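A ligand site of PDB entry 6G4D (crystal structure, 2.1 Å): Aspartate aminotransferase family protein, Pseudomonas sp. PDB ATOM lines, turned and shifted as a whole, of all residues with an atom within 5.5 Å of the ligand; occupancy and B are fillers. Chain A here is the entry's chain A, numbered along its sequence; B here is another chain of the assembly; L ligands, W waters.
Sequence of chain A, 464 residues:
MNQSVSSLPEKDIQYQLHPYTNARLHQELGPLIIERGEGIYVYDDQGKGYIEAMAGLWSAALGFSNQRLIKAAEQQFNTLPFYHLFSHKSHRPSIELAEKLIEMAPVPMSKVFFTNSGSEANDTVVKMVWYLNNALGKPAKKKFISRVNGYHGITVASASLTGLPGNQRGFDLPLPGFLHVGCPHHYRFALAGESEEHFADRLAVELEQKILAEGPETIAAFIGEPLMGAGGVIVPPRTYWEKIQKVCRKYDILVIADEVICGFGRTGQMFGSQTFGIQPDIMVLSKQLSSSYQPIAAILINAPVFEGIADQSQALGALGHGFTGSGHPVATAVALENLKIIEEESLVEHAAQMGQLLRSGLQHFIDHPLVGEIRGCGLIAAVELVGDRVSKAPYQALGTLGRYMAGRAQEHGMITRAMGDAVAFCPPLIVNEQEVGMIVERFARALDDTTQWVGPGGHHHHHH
N of Thr 324 of chain B lies within hydrogen-bond range of O3 of the ligand (2.8 Å).
OD2 of Asp 258 lies within hydrogen-bond range of N1 of the ligand (2.9 Å).
O4 of the ligand is in hydrogen-bond range of N of Gly 118 (3.0 Å).
The side-chain hydroxyl of Ser 119 is in hydrogen-bond range of an oxygen (O5) of the ligand, 2.5 Å away.
A carbon (C5) of the ligand is bonded to the side-chain amino group (NZ) of Lys 287, at 1.5 Å.
The backbone NH of Ser 119 sits at hydrogen-bond distance from an oxygen (O5) of the ligand (2.8 Å).
An oxygen (O3) of the ligand is in hydrogen-bond range of the side-chain hydroxyl of Thr 324 of chain B, 2.7 Å away.
N of Ser 117 lies within hydrogen-bond range of OE1 of Glu 120 of chain A, at 3.0 Å.
The side-chain hydroxyl (OG) of Ser 117 sits at hydrogen-bond distance from the side-chain carboxylate (OE2) of Glu 120 of chain B (2.5 Å).
OD2 of Asp 258 sits at hydrogen-bond distance from ND1 of His 152 (2.8 Å).
The side-chain hydroxyl (OG) of Ser 119 lies within hydrogen-bond range of the backbone NH (N) of Ile 154 (2.9 Å).
The side-chain carboxylate of Asp 258 is in hydrogen-bond range of the backbone NH of Val 260 (3.0 Å).
N of Tyr 151 sits at hydrogen-bond distance from OE2 of Glu 225.
The backbone carbonyl oxygen of His 152 is in hydrogen-bond range of the side-chain amide nitrogen of Asn 122, 2.9 Å away.
The side-chain carboxylate of Asp 258 lies within hydrogen-bond range of the side-chain amide nitrogen of Asn 122 (3.0 Å).
O of Tyr 151 sits close to N1 of the ligand, at 3.4 Å.
Merely in contact with the ligand: Ile 261, Val 260, Glu 225, Ser 117, His 152, Phe 323 of chain B and Gly 153.
Hydrophobic or aromatic side chains within 4 Å of the ligand: Tyr 151, Val 260, Ile 261 and Phe 323 of chain B.
13 residues have an atom within 4 Å of the ligand: Ser 117, Gly 118, Ser 119, Tyr 151, His 152, Gly 153, Glu 225, Asp 258, Val 260, Ile 261, Lys 287, Phe 323 of chain B and Thr 324 of chain B.
Water W2 lies within hydrogen-bond range of OH of Tyr 151 (2.6 Å), O3 of the ligand (2.7 Å) and O of Gly 322 of chain B (2.9 Å).
Water W3 bridges O4 of the ligand and OG of Ser 286.
Water W1 lies within hydrogen-bond range of OE1 of Glu 225, O1 of the ligand and N of Ala 230.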
ATOM      1  N   TRP A  58      22.330  15.988 -17.338  1.00  0.00           N
ATOM      2  CA  TRP A  58      21.826  17.157 -16.610  1.00  0.00           C
ATOM      3  C   TRP A  58      22.846  17.649 -15.561  1.00  0.00           C
ATOM      4  O   TRP A  58      22.445  18.296 -14.587  1.00  0.00           O
ATOM      5  CB  TRP A  58      20.481  16.870 -15.910  1.00  0.00           C
ATOM      6  CG  TRP A  58      19.452  16.041 -16.633  1.00  0.00           C
ATOM      7  CD1 TRP A  58      19.424  14.661 -16.727  1.00  0.00           C
ATOM      8  CD2 TRP A  58      18.247  16.506 -17.294  1.00  0.00           C
ATOM      9  NE1 TRP A  58      18.304  14.251 -17.435  1.00  0.00           N
ATOM     10  CE2 TRP A  58      17.572  15.353 -17.782  1.00  0.00           C
ATOM     11  CE3 TRP A  58      17.684  17.753 -17.511  1.00  0.00           C
ATOM     12  CZ2 TRP A  58      16.376  15.436 -18.500  1.00  0.00           C
ATOM     13  CZ3 TRP A  58      16.492  17.840 -18.213  1.00  0.00           C
ATOM     14  CH2 TRP A  58      15.853  16.684 -18.702  1.00  0.00           C
ATOM     15  N   ASN A 116      26.795   8.032  -2.869  1.00  0.00           N
ATOM     16  CA  ASN A 116      27.401   8.067  -4.201  1.00  0.00           C
ATOM     17  C   ASN A 116      26.430   8.631  -5.222  1.00  0.00           C
ATOM     18  O   ASN A 116      26.806   9.443  -6.046  1.00  0.00           O
ATOM     19  CB  ASN A 116      27.857   6.682  -4.674  1.00  0.00           C
ATOM     20  CG  ASN A 116      28.782   5.986  -3.694  1.00  0.00           C
ATOM     21  OD1 ASN A 116      29.939   6.389  -3.507  1.00  0.00           O
ATOM     22  ND2 ASN A 116      28.277   4.935  -3.045  1.00  0.00           N
ATOM     23  N   SER A 117      25.174   8.206  -5.156  1.00  0.00           N
ATOM     24  CA  SER A 117      24.212   8.602  -6.170  1.00  0.00           C
ATOM     25  C   SER A 117      22.976   9.242  -5.588  1.00  0.00           C
ATOM     26  O   SER A 117      22.671   9.095  -4.397  1.00  0.00           O
ATOM     27  CB  SER A 117      23.770   7.368  -6.932  1.00  0.00           C
ATOM     28  OG  SER A 117      23.059   6.500  -6.078  1.00  0.00           O
ATOM     29  N   GLY A 118      22.236   9.926  -6.459  1.00  0.00           N
ATOM     30  CA  GLY A 118      20.930  10.491  -6.142  1.00  0.00           C
ATOM     31  C   GLY A 118      19.937   9.441  -5.710  1.00  0.00           C
ATOM     32  O   GLY A 118      19.131   9.660  -4.788  1.00  0.00           O
ATOM     33  N   SER A 119      19.974   8.285  -6.384  1.00  0.00           N
ATOM     34  CA  SER A 119      19.052   7.215  -6.049  1.00  0.00           C
ATOM     35  C   SER A 119      19.350   6.720  -4.652  1.00  0.00           C
ATOM     36  O   SER A 119      18.416   6.458  -3.904  1.00  0.00           O
ATOM     37  CB  SER A 119      19.178   6.048  -7.021  1.00  0.00           C
ATOM     38  OG  SER A 119      18.860   6.417  -8.352  1.00  0.00           O
ATOM     39  N   GLU A 120      20.622   6.521  -4.315  1.00  0.00           N
ATOM     40  CA  GLU A 120      21.014   6.107  -2.951  1.00  0.00           C
ATOM     41  C   GLU A 120      20.588   7.127  -1.896  1.00  0.00           C
ATOM     42  O   GLU A 120      20.164   6.766  -0.813  1.00  0.00           O
ATOM     43  CB  GLU A 120      22.524   5.959  -2.839  1.00  0.00           C
ATOM     44  CG  GLU A 120      23.167   4.680  -3.348  1.00  0.00           C
ATOM     45  CD  GLU A 120      24.709   4.814  -3.313  1.00  0.00           C
ATOM     46  OE1 GLU A 120      25.201   5.950  -3.196  1.00  0.00           O
ATOM     47  OE2 GLU A 120      25.417   3.796  -3.432  1.00  0.00           O
ATOM     48  N   ASN A 122      18.023   9.328  -2.000  1.00  0.00           N
ATOM     49  CA  ASN A 122      16.587   9.267  -1.772  1.00  0.00           C
ATOM     50  C   ASN A 122      16.202   7.985  -1.050  1.00  0.00           C
ATOM     51  O   ASN A 122      15.292   8.008  -0.232  1.00  0.00           O
ATOM     52  CB  ASN A 122      15.787   9.438  -3.086  1.00  0.00           C
ATOM     53  CG  ASN A 122      15.721  10.888  -3.536  1.00  0.00           C
ATOM     54  OD1 ASN A 122      15.674  11.797  -2.693  1.00  0.00           O
ATOM     55  ND2 ASN A 122      15.744  11.112  -4.840  1.00  0.00           N
ATOM     56  N   TYR A 151      10.866  12.048 -10.990  1.00  0.00           N
ATOM     57  CA  TYR A 151      11.975  11.092 -11.041  1.00  0.00           C
ATOM     58  C   TYR A 151      12.864  11.288  -9.810  1.00  0.00           C
ATOM     59  O   TYR A 151      13.304  12.385  -9.516  1.00  0.00           O
ATOM     60  CB  TYR A 151      12.789  11.225 -12.321  1.00  0.00           C
ATOM     61  CG  TYR A 151      13.887  10.183 -12.449  1.00  0.00           C
ATOM     62  CD1 TYR A 151      13.587   8.886 -12.797  1.00  0.00           C
ATOM     63  CD2 TYR A 151      15.223  10.501 -12.209  1.00  0.00           C
ATOM     64  CE1 TYR A 151      14.564   7.928 -12.913  1.00  0.00           C
ATOM     65  CE2 TYR A 151      16.208   9.539 -12.320  1.00  0.00           C
ATOM     66  CZ  TYR A 151      15.870   8.251 -12.679  1.00  0.00           C
ATOM     67  OH  TYR A 151      16.826   7.295 -12.820  1.00  0.00           O
ATOM     68  N   HIS A 152      13.065  10.221  -9.066  1.00  0.00           N
ATOM     69  CA  HIS A 152      13.826  10.296  -7.828  1.00  0.00           C
ATOM     70  C   HIS A 152      14.821   9.170  -7.715  1.00  0.00           C
ATOM     71  O   HIS A 152      15.352   8.927  -6.648  1.00  0.00           O
ATOM     72  CB  HIS A 152      12.875  10.257  -6.632  1.00  0.00           C
ATOM     73  CG  HIS A 152      11.883  11.357  -6.638  1.00  0.00           C
ATOM     74  ND1 HIS A 152      12.250  12.664  -6.405  1.00  0.00           N
ATOM     75  CD2 HIS A 152      10.567  11.373  -6.945  1.00  0.00           C
ATOM     76  CE1 HIS A 152      11.186  13.440  -6.503  1.00  0.00           C
ATOM     77  NE2 HIS A 152      10.155  12.682  -6.835  1.00  0.00           N
ATOM     78  N   GLY A 153      15.121   8.510  -8.838  1.00  0.00           N
ATOM     79  CA  GLY A 153      16.125   7.467  -8.840  1.00  0.00           C
ATOM     80  C   GLY A 153      15.516   6.111  -9.054  1.00  0.00           C
ATOM     81  O   GLY A 153      14.323   5.990  -9.302  1.00  0.00           O
ATOM     82  N   ILE A 154      16.361   5.089  -8.992  1.00  0.00           N
ATOM     83  CA  ILE A 154      15.984   3.763  -9.455  1.00  0.00           C
ATOM     84  C   ILE A 154      16.381   2.577  -8.557  1.00  0.00           C
ATOM     85  O   ILE A 154      16.336   1.425  -8.996  1.00  0.00           O
ATOM     86  CB  ILE A 154      16.443   3.549 -10.912  1.00  0.00           C
ATOM     87  CG1 ILE A 154      17.840   4.092 -11.180  1.00  0.00           C
ATOM     88  CG2 ILE A 154      15.497   4.276 -11.858  1.00  0.00           C
ATOM     89  CD1 ILE A 154      18.957   3.251 -10.616  1.00  0.00           C
ATOM     90  N   GLU A 225      10.807  17.280  -6.912  1.00  0.00           N
ATOM     91  CA  GLU A 225      11.755  18.147  -7.593  1.00  0.00           C
ATOM     92  C   GLU A 225      11.066  19.513  -7.701  1.00  0.00           C
ATOM     93  O   GLU A 225       9.883  19.554  -7.996  1.00  0.00           O
ATOM     94  CB  GLU A 225      12.007  17.641  -9.008  1.00  0.00           C
ATOM     95  CG  GLU A 225      12.517  16.219  -9.105  1.00  0.00           C
ATOM     96  CD  GLU A 225      12.227  15.614 -10.444  1.00  0.00           C
ATOM     97  OE1 GLU A 225      13.056  15.794 -11.356  1.00  0.00           O
ATOM     98  OE2 GLU A 225      11.144  14.983 -10.602  1.00  0.00           O
ATOM     99  N   ALA A 230      13.691  14.794 -15.557  1.00  0.00           N
ATOM    100  CA  ALA A 230      13.587  13.663 -16.457  1.00  0.00           C
ATOM    101  C   ALA A 230      12.190  13.418 -16.952  1.00  0.00           C
ATOM    102  O   ALA A 230      11.997  12.799 -17.978  1.00  0.00           O
ATOM    103  CB  ALA A 230      14.092  12.397 -15.781  1.00  0.00           C
ATOM    104  N   ASP A 258      13.820  17.434  -3.788  1.00  0.00           N
ATOM    105  CA  ASP A 258      14.811  16.712  -4.604  1.00  0.00           C
ATOM    106  C   ASP A 258      15.424  17.703  -5.593  1.00  0.00           C
ATOM    107  O   ASP A 258      14.857  17.983  -6.659  1.00  0.00           O
ATOM    108  CB  ASP A 258      14.167  15.538  -5.330  1.00  0.00           C
ATOM    109  CG  ASP A 258      15.177  14.682  -6.068  1.00  0.00           C
ATOM    110  OD1 ASP A 258      16.258  15.210  -6.379  1.00  0.00           O
ATOM    111  OD2 ASP A 258      14.885  13.501  -6.356  1.00  0.00           O
ATOM    112  N   VAL A 260      18.321  17.246  -7.164  1.00  0.00           N
ATOM    113  CA  VAL A 260      19.383  16.557  -7.870  1.00  0.00           C
ATOM    114  C   VAL A 260      19.692  17.241  -9.190  1.00  0.00           C
ATOM    115  O   VAL A 260      20.849  17.389  -9.550  1.00  0.00           O
ATOM    116  CB  VAL A 260      19.079  15.054  -7.993  1.00  0.00           C
ATOM    117  CG1 VAL A 260      19.892  14.388  -9.098  1.00  0.00           C
ATOM    118  CG2 VAL A 260      19.371  14.386  -6.650  1.00  0.00           C
ATOM    119  N   ILE A 261      18.664  17.678  -9.930  1.00  0.00           N
ATOM    120  CA  ILE A 261      18.876  18.448 -11.172  1.00  0.00           C
ATOM    121  C   ILE A 261      18.912  19.967 -10.922  1.00  0.00           C
ATOM    122  O   ILE A 261      19.772  20.661 -11.486  1.00  0.00           O
ATOM    123  CB  ILE A 261      17.832  18.106 -12.258  1.00  0.00           C
ATOM    124  CG1 ILE A 261      18.224  16.772 -12.908  1.00  0.00           C
ATOM    125  CG2 ILE A 261      17.796  19.183 -13.316  1.00  0.00           C
ATOM    126  CD1 ILE A 261      17.161  16.210 -13.835  1.00  0.00           C
ATOM    127  N   SER A 286      22.945  16.225  -5.952  1.00  0.00           N
ATOM    128  CA  SER A 286      23.907  15.390  -6.677  1.00  0.00           C
ATOM    129  C   SER A 286      24.269  16.099  -7.991  1.00  0.00           C
ATOM    130  O   SER A 286      24.184  17.334  -8.065  1.00  0.00           O
ATOM    131  CB  SER A 286      23.346  14.003  -6.932  1.00  0.00           C
ATOM    132  OG  SER A 286      24.357  13.100  -7.333  1.00  0.00           O
ATOM    133  N   LYS A 287      24.711  15.334  -9.005  1.00  0.00           N
ATOM    134  CA  LYS A 287      24.865  15.825 -10.400  1.00  0.00           C
ATOM    135  C   LYS A 287      25.778  17.040 -10.436  1.00  0.00           C
ATOM    136  O   LYS A 287      27.009  16.883 -10.364  1.00  0.00           O
ATOM    137  CB  LYS A 287      23.509  16.020 -11.085  1.00  0.00           C
ATOM    138  CG  LYS A 287      22.909  14.675 -11.503  1.00  0.00           C
ATOM    139  CD  LYS A 287      21.593  14.739 -12.297  1.00  0.00           C
ATOM    140  CE  LYS A 287      21.146  13.342 -12.808  1.00  0.00           C
ATOM    141  NZ  LYS A 287      19.735  13.026 -12.480  1.00  0.00           N
ATOM    142  N   ASN B 116      27.643   2.352  -8.799  1.00  0.00           N
ATOM    143  CA  ASN B 116      28.616   3.020  -7.945  1.00  0.00           C
ATOM    144  C   ASN B 116      29.006   2.182  -6.711  1.00  0.00           C
ATOM    145  O   ASN B 116      30.175   2.084  -6.382  1.00  0.00           O
ATOM    146  CB  ASN B 116      28.108   4.366  -7.444  1.00  0.00           C
ATOM    147  CG  ASN B 116      27.642   5.264  -8.569  1.00  0.00           C
ATOM    148  OD1 ASN B 116      28.449   5.735  -9.390  1.00  0.00           O
ATOM    149  ND2 ASN B 116      26.339   5.492  -8.638  1.00  0.00           N
ATOM    150  N   GLU B 120      24.009  -0.633  -4.148  1.00  0.00           N
ATOM    151  CA  GLU B 120      23.296  -0.379  -5.397  1.00  0.00           C
ATOM    152  C   GLU B 120      23.293  -1.606  -6.302  1.00  0.00           C
ATOM    153  O   GLU B 120      22.279  -1.906  -6.961  1.00  0.00           O
ATOM    154  CB  GLU B 120      23.950   0.741  -6.186  1.00  0.00           C
ATOM    155  CG  GLU B 120      23.640   2.170  -5.799  1.00  0.00           C
ATOM    156  CD  GLU B 120      24.527   3.134  -6.588  1.00  0.00           C
ATOM    157  OE1 GLU B 120      25.530   2.672  -7.199  1.00  0.00           O
ATOM    158  OE2 GLU B 120      24.236   4.358  -6.641  1.00  0.00           O
ATOM    159  N   GLY B 322      19.327   2.455 -14.493  1.00  0.00           N
ATOM    160  CA  GLY B 322      20.672   2.954 -14.673  1.00  0.00           C
ATOM    161  C   GLY B 322      20.976   4.136 -13.758  1.00  0.00           C
ATOM    162  O   GLY B 322      20.115   4.998 -13.523  1.00  0.00           O
ATOM    163  N   PHE B 323      22.195   4.196 -13.250  1.00  0.00           N
ATOM    164  CA  PHE B 323      22.655   5.295 -12.410  1.00  0.00           C
ATOM    165  C   PHE B 323      23.455   6.260 -13.257  1.00  0.00           C
ATOM    166  O   PHE B 323      24.126   5.856 -14.224  1.00  0.00           O
ATOM    167  CB  PHE B 323      23.534   4.762 -11.288  1.00  0.00           C
ATOM    168  CG  PHE B 323      22.850   3.762 -10.413  1.00  0.00           C
ATOM    169  CD1 PHE B 323      22.083   4.180  -9.329  1.00  0.00           C
ATOM    170  CD2 PHE B 323      22.932   2.406 -10.688  1.00  0.00           C
ATOM    171  CE1 PHE B 323      21.443   3.245  -8.514  1.00  0.00           C
ATOM    172  CE2 PHE B 323      22.280   1.480  -9.890  1.00  0.00           C
ATOM    173  CZ  PHE B 323      21.535   1.895  -8.805  1.00  0.00           C
ATOM    174  N   THR B 324      23.382   7.542 -12.914  1.00  0.00           N
ATOM    175  CA  THR B 324      24.195   8.550 -13.585  1.00  0.00           C
ATOM    176  C   THR B 324      25.655   8.116 -13.712  1.00  0.00           C
ATOM    177  O   THR B 324      26.246   8.231 -14.772  1.00  0.00           O
ATOM    178  CB  THR B 324      24.094   9.893 -12.873  1.00  0.00           C
ATOM    179  OG1 THR B 324      22.745  10.351 -12.978  1.00  0.00           O
ATOM    180  CG2 THR B 324      25.044  10.949 -13.484  1.00  0.00           C
ATOM    181  N   GLY B 325      26.190   7.550 -12.635  1.00  0.00           N
ATOM    182  CA  GLY B 325      27.595   7.168 -12.565  1.00  0.00           C
ATOM    183  C   GLY B 325      27.891   5.767 -13.039  1.00  0.00           C
ATOM    184  O   GLY B 325      29.060   5.338 -12.958  1.00  0.00           O
HETATM  185  N1  LIG L   1      16.543  12.618  -8.520  1.00  0.00           N
HETATM  186  C1  LIG L   1      16.524  13.429  -9.600  1.00  0.00           C
HETATM  187  C2  LIG L   1      15.626  14.625  -9.673  1.00  0.00           C
HETATM  188  C3  LIG L   1      17.373  13.115 -10.767  1.00  0.00           C
HETATM  189  O1  LIG L   1      17.306  13.895 -11.866  1.00  0.00           O
HETATM  190  C4  LIG L   1      18.285  11.957 -10.760  1.00  0.00           C
HETATM  191  C5  LIG L   1      19.190  11.733 -11.995  1.00  0.00           C
HETATM  192  C6  LIG L   1      18.239  11.140  -9.524  1.00  0.00           C
HETATM  193  C7  LIG L   1      17.362  11.520  -8.479  1.00  0.00           C
HETATM  194  C8  LIG L   1      19.077   9.870  -9.344  1.00  0.00           C
HETATM  195  O2  LIG L   1      20.466  10.065  -9.491  1.00  0.00           O
HETATM  196  P1  LIG L   1      21.468   8.838  -9.776  1.00  0.00           P
HETATM  197  O3  LIG L   1      21.423   8.718 -11.277  1.00  0.00           O
HETATM  198  O4  LIG L   1      22.821   9.415  -9.405  1.00  0.00           O
HETATM  199  O5  LIG L   1      20.983   7.676  -8.951  1.00  0.00           O
HETATM  200  O   HOH W   1      14.604  14.102 -12.892  1.00  0.00           O
HETATM  201  O   HOH W   2      19.360   7.671 -12.617  1.00  0.00           O
HETATM  202  O   HOH W   3      24.495  11.518  -9.597  1.00  0.00           O
HETATM  203  O   HOH W   4      24.973   7.937  -9.961  1.00  0.00           O
